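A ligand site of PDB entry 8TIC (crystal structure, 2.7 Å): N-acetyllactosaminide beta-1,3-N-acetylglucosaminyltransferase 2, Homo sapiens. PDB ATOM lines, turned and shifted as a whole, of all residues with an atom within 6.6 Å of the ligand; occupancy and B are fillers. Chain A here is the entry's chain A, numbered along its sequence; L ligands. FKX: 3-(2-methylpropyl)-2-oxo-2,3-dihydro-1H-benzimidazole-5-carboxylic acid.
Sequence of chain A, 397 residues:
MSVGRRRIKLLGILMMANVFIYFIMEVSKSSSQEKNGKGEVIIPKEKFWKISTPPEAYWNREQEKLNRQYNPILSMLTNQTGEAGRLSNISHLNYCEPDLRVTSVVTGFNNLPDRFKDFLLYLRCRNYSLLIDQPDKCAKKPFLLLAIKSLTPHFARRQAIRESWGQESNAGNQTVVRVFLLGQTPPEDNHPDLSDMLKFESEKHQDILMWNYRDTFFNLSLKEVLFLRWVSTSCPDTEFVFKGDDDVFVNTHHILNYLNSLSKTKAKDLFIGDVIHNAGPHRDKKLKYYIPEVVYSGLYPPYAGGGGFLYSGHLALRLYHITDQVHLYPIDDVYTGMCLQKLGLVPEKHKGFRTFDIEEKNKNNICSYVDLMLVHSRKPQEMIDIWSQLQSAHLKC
Merely in contact with the ligand: Phe 217 (3.3 Å), Lys 149 (3.4 Å), Asp 245 (3.5 Å), Asp 246 (3.6 Å), Leu 220 (3.6 Å), Thr 216 (3.6 Å), Leu 151 (3.7 Å) and Asp 247 (3.7 Å). 12 residues have an atom within 4 Å of the ligand: Lys 149, Ser 150, Leu 151, Asp 215, Thr 216, Phe 217, Leu 220, Lys 223, Asp 245, Asp 246, Asp 247 and Lys 288. The nearest printed residue that does not touch the ligand is His 154 (4.002 Å).
NZ of Lys 223 sits at hydrogen-bond distance from O12 of the ligand. An oxygen (O05) of the ligand is in salt-bridge range of the side-chain amino group (NZ) of Lys 288, 2.8 Å away. The side-chain carboxylate of Asp 215 is in hydrogen-bond range of a nitrogen (N10) of the ligand, 3.0 Å away. N of Ser 150 sits at hydrogen-bond distance from O12 of the ligand, at 3.5 Å.
The backbone carbonyl oxygen of Ser 150 sits at hydrogen-bond distance from the side-chain amino group of Lys 223 (3.3 Å). The side-chain amino group (NZ) of Lys 223 sits close to the backbone carbonyl oxygen (O) of Leu 181 (3.3 Å). The side-chain carboxylate (OD2) of Asp 215 sits at hydrogen-bond distance from the backbone NH (N) of Gly 183 (3.0 Å). OG of Ser 150 is in hydrogen-bond range of OD2 of Asp 246 (3.1 Å). N of Ser 150 lies within hydrogen-bond range of O of Leu 181, at 3.2 Å. The side-chain amino group of Lys 149 lies within salt-bridge range of the side-chain carboxylate of Asp 245 (3.4 Å). O of Gly 244 lies within hydrogen-bond range of N of Lys 149, 2.6 Å away. The guanidinium group (NH1) of Arg 157 lies within salt-bridge range of the side-chain carboxylate (OD1) of Asp 246 (2.6 Å).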
ATOM      1  N   ILE A 148     -28.203 -20.848  11.886  1.00  0.00           N
ATOM      2  CA  ILE A 148     -28.387 -19.453  11.487  1.00  0.00           C
ATOM      3  C   ILE A 148     -27.021 -18.835  11.299  1.00  0.00           C
ATOM      4  O   ILE A 148     -26.210 -18.810  12.237  1.00  0.00           O
ATOM      5  CB  ILE A 148     -29.207 -18.676  12.528  1.00  0.00           C
ATOM      6  CG1 ILE A 148     -30.240 -19.594  13.187  1.00  0.00           C
ATOM      7  CG2 ILE A 148     -29.864 -17.460  11.890  1.00  0.00           C
ATOM      8  CD1 ILE A 148     -31.319 -20.045  12.251  1.00  0.00           C
ATOM      9  N   LYS A 149     -26.757 -18.326  10.105  1.00  0.00           N
ATOM     10  CA  LYS A 149     -25.552 -17.552   9.874  1.00  0.00           C
ATOM     11  C   LYS A 149     -25.666 -16.214  10.609  1.00  0.00           C
ATOM     12  O   LYS A 149     -26.660 -15.488  10.441  1.00  0.00           O
ATOM     13  CB  LYS A 149     -25.340 -17.311   8.379  1.00  0.00           C
ATOM     14  CG  LYS A 149     -25.048 -18.550   7.559  1.00  0.00           C
ATOM     15  CD  LYS A 149     -24.702 -18.152   6.129  1.00  0.00           C
ATOM     16  CE  LYS A 149     -25.937 -18.108   5.242  1.00  0.00           C
ATOM     17  NZ  LYS A 149     -25.630 -17.774   3.822  1.00  0.00           N
ATOM     18  N   SER A 150     -24.661 -15.893  11.411  1.00  0.00           N
ATOM     19  CA  SER A 150     -24.634 -14.648  12.159  1.00  0.00           C
ATOM     20  C   SER A 150     -23.208 -14.106  12.229  1.00  0.00           C
ATOM     21  O   SER A 150     -22.243 -14.810  11.942  1.00  0.00           O
ATOM     22  CB  SER A 150     -25.189 -14.831  13.583  1.00  0.00           C
ATOM     23  OG  SER A 150     -25.302 -13.591  14.253  1.00  0.00           O
ATOM     24  N   LEU A 151     -23.099 -12.841  12.622  1.00  0.00           N
ATOM     25  CA  LEU A 151     -21.840 -12.171  12.893  1.00  0.00           C
ATOM     26  C   LEU A 151     -21.764 -11.816  14.380  1.00  0.00           C
ATOM     27  O   LEU A 151     -22.784 -11.701  15.065  1.00  0.00           O
ATOM     28  CB  LEU A 151     -21.699 -10.906  12.049  1.00  0.00           C
ATOM     29  CG  LEU A 151     -21.212 -11.081  10.605  1.00  0.00           C
ATOM     30  CD1 LEU A 151     -21.377  -9.783   9.835  1.00  0.00           C
ATOM     31  CD2 LEU A 151     -19.760 -11.539  10.575  1.00  0.00           C
ATOM     32  N   HIS A 154     -24.068  -9.158  16.241  1.00  0.00           N
ATOM     33  CA  HIS A 154     -25.517  -9.237  16.060  1.00  0.00           C
ATOM     34  C   HIS A 154     -26.209  -9.878  17.263  1.00  0.00           C
ATOM     35  O   HIS A 154     -26.988 -10.815  17.129  1.00  0.00           O
ATOM     36  CB  HIS A 154     -25.822 -10.013  14.784  1.00  0.00           C
ATOM     37  CG  HIS A 154     -25.352  -9.319  13.540  1.00  0.00           C
ATOM     38  ND1 HIS A 154     -25.550  -9.836  12.279  1.00  0.00           N
ATOM     39  CD2 HIS A 154     -24.689  -8.154  13.361  1.00  0.00           C
ATOM     40  CE1 HIS A 154     -25.033  -9.018  11.374  1.00  0.00           C
ATOM     41  NE2 HIS A 154     -24.497  -7.991  12.009  1.00  0.00           N
ATOM     42  N   ARG A 157     -30.058  -9.572  16.902  1.00  0.00           N
ATOM     43  CA  ARG A 157     -30.648 -10.450  15.897  1.00  0.00           C
ATOM     44  C   ARG A 157     -30.768 -11.873  16.434  1.00  0.00           C
ATOM     45  O   ARG A 157     -31.810 -12.522  16.290  1.00  0.00           O
ATOM     46  CB  ARG A 157     -29.814 -10.425  14.621  1.00  0.00           C
ATOM     47  CG  ARG A 157     -30.019  -9.201  13.746  1.00  0.00           C
ATOM     48  CD  ARG A 157     -29.247  -9.402  12.466  1.00  0.00           C
ATOM     49  NE  ARG A 157     -29.094  -8.197  11.665  1.00  0.00           N
ATOM     50  CZ  ARG A 157     -28.571  -8.177  10.439  1.00  0.00           C
ATOM     51  NH1 ARG A 157     -28.163  -9.282   9.856  1.00  0.00           N
ATOM     52  NH2 ARG A 157     -28.453  -7.020   9.803  1.00  0.00           N
ATOM     53  N   LEU A 181     -23.919 -19.767  13.512  1.00  0.00           N
ATOM     54  CA  LEU A 181     -22.652 -20.046  12.852  1.00  0.00           C
ATOM     55  C   LEU A 181     -21.824 -18.767  12.761  1.00  0.00           C
ATOM     56  O   LEU A 181     -22.174 -17.843  12.015  1.00  0.00           O
ATOM     57  CB  LEU A 181     -22.891 -20.610  11.454  1.00  0.00           C
ATOM     58  CG  LEU A 181     -23.868 -21.776  11.372  1.00  0.00           C
ATOM     59  CD1 LEU A 181     -24.153 -22.104   9.920  1.00  0.00           C
ATOM     60  CD2 LEU A 181     -23.318 -22.984  12.119  1.00  0.00           C
ATOM     61  N   LEU A 182     -20.709 -18.718  13.488  1.00  0.00           N
ATOM     62  CA  LEU A 182     -19.861 -17.535  13.532  1.00  0.00           C
ATOM     63  C   LEU A 182     -18.430 -17.869  13.165  1.00  0.00           C
ATOM     64  O   LEU A 182     -17.928 -18.949  13.461  1.00  0.00           O
ATOM     65  CB  LEU A 182     -19.870 -16.888  14.933  1.00  0.00           C
ATOM     66  CG  LEU A 182     -21.023 -15.947  15.282  1.00  0.00           C
ATOM     67  CD1 LEU A 182     -22.283 -16.726  15.587  1.00  0.00           C
ATOM     68  CD2 LEU A 182     -20.663 -15.059  16.448  1.00  0.00           C
ATOM     69  N   GLY A 183     -17.777 -16.909  12.521  1.00  0.00           N
ATOM     70  CA  GLY A 183     -16.329 -16.874  12.402  1.00  0.00           C
ATOM     71  C   GLY A 183     -15.730 -15.913  13.408  1.00  0.00           C
ATOM     72  O   GLY A 183     -16.177 -15.826  14.553  1.00  0.00           O
ATOM     73  N   TYR A 213     -11.674 -18.600  11.588  1.00  0.00           N
ATOM     74  CA  TYR A 213     -11.430 -17.980  10.303  1.00  0.00           C
ATOM     75  C   TYR A 213     -12.036 -16.580  10.268  1.00  0.00           C
ATOM     76  O   TYR A 213     -12.889 -16.210  11.084  1.00  0.00           O
ATOM     77  CB  TYR A 213     -11.978 -18.848   9.176  1.00  0.00           C
ATOM     78  CG  TYR A 213     -13.452 -18.906   9.140  1.00  0.00           C
ATOM     79  CD1 TYR A 213     -14.146 -19.761   9.984  1.00  0.00           C
ATOM     80  CD2 TYR A 213     -14.171 -18.106   8.273  1.00  0.00           C
ATOM     81  CE1 TYR A 213     -15.514 -19.809   9.957  1.00  0.00           C
ATOM     82  CE2 TYR A 213     -15.533 -18.145   8.230  1.00  0.00           C
ATOM     83  CZ  TYR A 213     -16.203 -19.001   9.070  1.00  0.00           C
ATOM     84  OH  TYR A 213     -17.572 -19.049   9.043  1.00  0.00           O
ATOM     85  N   ASP A 215     -14.382 -14.107   9.465  1.00  0.00           N
ATOM     86  CA  ASP A 215     -15.758 -14.110   9.003  1.00  0.00           C
ATOM     87  C   ASP A 215     -15.996 -12.929   8.068  1.00  0.00           C
ATOM     88  O   ASP A 215     -16.394 -11.855   8.517  1.00  0.00           O
ATOM     89  CB  ASP A 215     -16.731 -14.082  10.174  1.00  0.00           C
ATOM     90  CG  ASP A 215     -18.131 -14.528   9.794  1.00  0.00           C
ATOM     91  OD1 ASP A 215     -18.418 -14.630   8.586  1.00  0.00           O
ATOM     92  OD2 ASP A 215     -18.940 -14.776  10.704  1.00  0.00           O
ATOM     93  N   THR A 216     -15.746 -13.117   6.783  1.00  0.00           N
ATOM     94  CA  THR A 216     -16.007 -12.100   5.785  1.00  0.00           C
ATOM     95  C   THR A 216     -16.969 -12.638   4.747  1.00  0.00           C
ATOM     96  O   THR A 216     -17.259 -13.842   4.681  1.00  0.00           O
ATOM     97  CB  THR A 216     -14.709 -11.661   5.101  1.00  0.00           C
ATOM     98  OG1 THR A 216     -14.194 -12.749   4.327  1.00  0.00           O
ATOM     99  CG2 THR A 216     -13.667 -11.239   6.128  1.00  0.00           C
ATOM    100  N   PHE A 217     -17.463 -11.724   3.906  1.00  0.00           N
ATOM    101  CA  PHE A 217     -18.478 -12.072   2.918  1.00  0.00           C
ATOM    102  C   PHE A 217     -17.986 -13.180   1.981  1.00  0.00           C
ATOM    103  O   PHE A 217     -18.745 -14.107   1.679  1.00  0.00           O
ATOM    104  CB  PHE A 217     -18.871 -10.826   2.131  1.00  0.00           C
ATOM    105  CG  PHE A 217     -19.868 -11.068   1.040  1.00  0.00           C
ATOM    106  CD1 PHE A 217     -21.119 -11.616   1.320  1.00  0.00           C
ATOM    107  CD2 PHE A 217     -19.580 -10.732  -0.266  1.00  0.00           C
ATOM    108  CE1 PHE A 217     -22.038 -11.821   0.314  1.00  0.00           C
ATOM    109  CE2 PHE A 217     -20.493 -10.941  -1.283  1.00  0.00           C
ATOM    110  CZ  PHE A 217     -21.729 -11.491  -0.987  1.00  0.00           C
ATOM    111  N   PHE A 218     -16.731 -13.112   1.544  1.00  0.00           N
ATOM    112  CA  PHE A 218     -16.212 -14.094   0.602  1.00  0.00           C
ATOM    113  C   PHE A 218     -15.790 -15.396   1.273  1.00  0.00           C
ATOM    114  O   PHE A 218     -15.467 -16.359   0.582  1.00  0.00           O
ATOM    115  CB  PHE A 218     -15.022 -13.525  -0.182  1.00  0.00           C
ATOM    116  CG  PHE A 218     -15.422 -12.776  -1.415  1.00  0.00           C
ATOM    117  CD1 PHE A 218     -16.745 -12.433  -1.653  1.00  0.00           C
ATOM    118  CD2 PHE A 218     -14.474 -12.410  -2.353  1.00  0.00           C
ATOM    119  CE1 PHE A 218     -17.105 -11.738  -2.782  1.00  0.00           C
ATOM    120  CE2 PHE A 218     -14.829 -11.719  -3.494  1.00  0.00           C
ATOM    121  CZ  PHE A 218     -16.152 -11.375  -3.707  1.00  0.00           C
ATOM    122  N   LEU A 220     -17.863 -17.101   3.167  1.00  0.00           N
ATOM    123  CA  LEU A 220     -19.100 -17.754   3.598  1.00  0.00           C
ATOM    124  C   LEU A 220     -19.177 -19.203   3.127  1.00  0.00           C
ATOM    125  O   LEU A 220     -19.834 -20.019   3.778  1.00  0.00           O
ATOM    126  CB  LEU A 220     -20.308 -16.963   3.099  1.00  0.00           C
ATOM    127  CG  LEU A 220     -20.722 -15.809   4.019  1.00  0.00           C
ATOM    128  CD1 LEU A 220     -21.826 -14.977   3.376  1.00  0.00           C
ATOM    129  CD2 LEU A 220     -21.139 -16.314   5.400  1.00  0.00           C
ATOM    130  N   LYS A 223     -17.825 -20.987   5.868  1.00  0.00           N
ATOM    131  CA  LYS A 223     -18.856 -21.145   6.890  1.00  0.00           C
ATOM    132  C   LYS A 223     -19.738 -22.343   6.586  1.00  0.00           C
ATOM    133  O   LYS A 223     -20.120 -23.101   7.490  1.00  0.00           O
ATOM    134  CB  LYS A 223     -19.685 -19.874   7.001  1.00  0.00           C
ATOM    135  CG  LYS A 223     -20.813 -19.946   8.011  1.00  0.00           C
ATOM    136  CD  LYS A 223     -21.361 -18.569   8.321  1.00  0.00           C
ATOM    137  CE  LYS A 223     -20.431 -17.804   9.255  1.00  0.00           C
ATOM    138  NZ  LYS A 223     -20.848 -16.384   9.384  1.00  0.00           N
ATOM    139  N   GLY A 244     -29.767 -20.581   7.216  1.00  0.00           N
ATOM    140  CA  GLY A 244     -30.099 -19.290   6.644  1.00  0.00           C
ATOM    141  C   GLY A 244     -29.502 -18.140   7.418  1.00  0.00           C
ATOM    142  O   GLY A 244     -28.704 -18.330   8.339  1.00  0.00           O
ATOM    143  N   ASP A 245     -29.907 -16.948   7.016  1.00  0.00           N
ATOM    144  CA  ASP A 245     -29.416 -15.687   7.548  1.00  0.00           C
ATOM    145  C   ASP A 245     -30.117 -15.353   8.869  1.00  0.00           C
ATOM    146  O   ASP A 245     -31.143 -15.934   9.225  1.00  0.00           O
ATOM    147  CB  ASP A 245     -29.635 -14.575   6.522  1.00  0.00           C
ATOM    148  CG  ASP A 245     -28.812 -14.773   5.250  1.00  0.00           C
ATOM    149  OD1 ASP A 245     -27.924 -15.657   5.219  1.00  0.00           O
ATOM    150  OD2 ASP A 245     -29.047 -14.027   4.267  1.00  0.00           O
ATOM    151  N   ASP A 246     -29.539 -14.402   9.609  1.00  0.00           N
ATOM    152  CA  ASP A 246     -30.128 -13.981  10.875  1.00  0.00           C
ATOM    153  C   ASP A 246     -31.085 -12.797  10.734  1.00  0.00           C
ATOM    154  O   ASP A 246     -31.656 -12.362  11.738  1.00  0.00           O
ATOM    155  CB  ASP A 246     -29.041 -13.648  11.905  1.00  0.00           C
ATOM    156  CG  ASP A 246     -28.135 -12.489  11.488  1.00  0.00           C
ATOM    157  OD1 ASP A 246     -28.418 -11.824  10.467  1.00  0.00           O
ATOM    158  OD2 ASP A 246     -27.141 -12.245  12.195  1.00  0.00           O
ATOM    159  N   ASP A 247     -31.263 -12.269   9.531  1.00  0.00           N
ATOM    160  CA  ASP A 247     -32.206 -11.190   9.301  1.00  0.00           C
ATOM    161  C   ASP A 247     -33.452 -11.661   8.544  1.00  0.00           C
ATOM    162  O   ASP A 247     -34.177 -10.841   7.975  1.00  0.00           O
ATOM    163  CB  ASP A 247     -31.526 -10.040   8.556  1.00  0.00           C
ATOM    164  CG  ASP A 247     -30.816 -10.479   7.301  1.00  0.00           C
ATOM    165  OD1 ASP A 247     -30.275 -11.606   7.284  1.00  0.00           O
ATOM    166  OD2 ASP A 247     -30.781  -9.695   6.319  1.00  0.00           O
ATOM    167  N   LYS A 288     -21.845  -5.730  -5.236  1.00  0.00           N
ATOM    168  CA  LYS A 288     -21.450  -6.630  -4.159  1.00  0.00           C
ATOM    169  C   LYS A 288     -21.126  -8.020  -4.679  1.00  0.00           C
ATOM    170  O   LYS A 288     -20.071  -8.583  -4.361  1.00  0.00           O
ATOM    171  CB  LYS A 288     -22.553  -6.702  -3.104  1.00  0.00           C
ATOM    172  CG  LYS A 288     -22.228  -7.618  -1.942  1.00  0.00           C
ATOM    173  CD  LYS A 288     -21.799  -6.817  -0.727  1.00  0.00           C
ATOM    174  CE  LYS A 288     -22.033  -7.599   0.543  1.00  0.00           C
ATOM    175  NZ  LYS A 288     -23.434  -8.076   0.639  1.00  0.00           N
ATOM    176  N   TYR A 289     -22.009  -8.592  -5.490  1.00  0.00           N
ATOM    177  CA  TYR A 289     -21.809  -9.929  -6.049  1.00  0.00           C
ATOM    178  C   TYR A 289     -20.992  -9.906  -7.334  1.00  0.00           C
ATOM    179  O   TYR A 289     -21.225 -10.735  -8.239  1.00  0.00           O
ATOM    180  CB  TYR A 289     -23.158 -10.610  -6.264  1.00  0.00           C
ATOM    181  CG  TYR A 289     -23.928 -10.801  -4.972  1.00  0.00           C
ATOM    182  CD1 TYR A 289     -24.775  -9.811  -4.483  1.00  0.00           C
ATOM    183  CD2 TYR A 289     -23.782 -11.967  -4.231  1.00  0.00           C
ATOM    184  CE1 TYR A 289     -25.466  -9.987  -3.297  1.00  0.00           C
ATOM    185  CE2 TYR A 289     -24.474 -12.156  -3.041  1.00  0.00           C
ATOM    186  CZ  TYR A 289     -25.308 -11.161  -2.580  1.00  0.00           C
ATOM    187  OH  TYR A 289     -25.999 -11.323  -1.399  1.00  0.00           O
HETATM  188  O12 FKX L   1     -22.750 -15.085   8.647  1.00  0.00           O
HETATM  189  N13 FKX L   1     -23.075 -13.239   7.016  1.00  0.00           N
HETATM  190  C14 FKX L   1     -24.495 -13.425   6.761  1.00  0.00           C
HETATM  191  C15 FKX L   1     -25.329 -12.360   7.488  1.00  0.00           C
HETATM  192  C16 FKX L   1     -26.798 -12.740   7.433  1.00  0.00           C
HETATM  193  C01 FKX L   1     -22.289 -12.170   6.360  1.00  0.00           C
HETATM  194  C02 FKX L   1     -22.568 -11.073   5.375  1.00  0.00           C
HETATM  195  C03 FKX L   1     -21.519 -10.211   4.967  1.00  0.00           C
HETATM  196  C04 FKX L   1     -21.792  -9.105   3.966  1.00  0.00           C
HETATM  197  C07 FKX L   1     -20.190 -10.392   5.501  1.00  0.00           C
HETATM  198  C08 FKX L   1     -19.908 -11.418   6.430  1.00  0.00           C
HETATM  199  C09 FKX L   1     -21.009 -12.323   6.868  1.00  0.00           C
HETATM  200  C11 FKX L   1     -22.349 -14.003   7.857  1.00  0.00           C
HETATM  201  C17 FKX L   1     -24.935 -12.206   8.957  1.00  0.00           C
HETATM  202  N10 FKX L   1     -21.111 -13.480   7.786  1.00  0.00           N
HETATM  203  O05 FKX L   1     -22.633  -9.313   3.059  1.00  0.00           O
HETATM  204  O06 FKX L   1     -21.146  -8.022   4.024  1.00  0.00           O
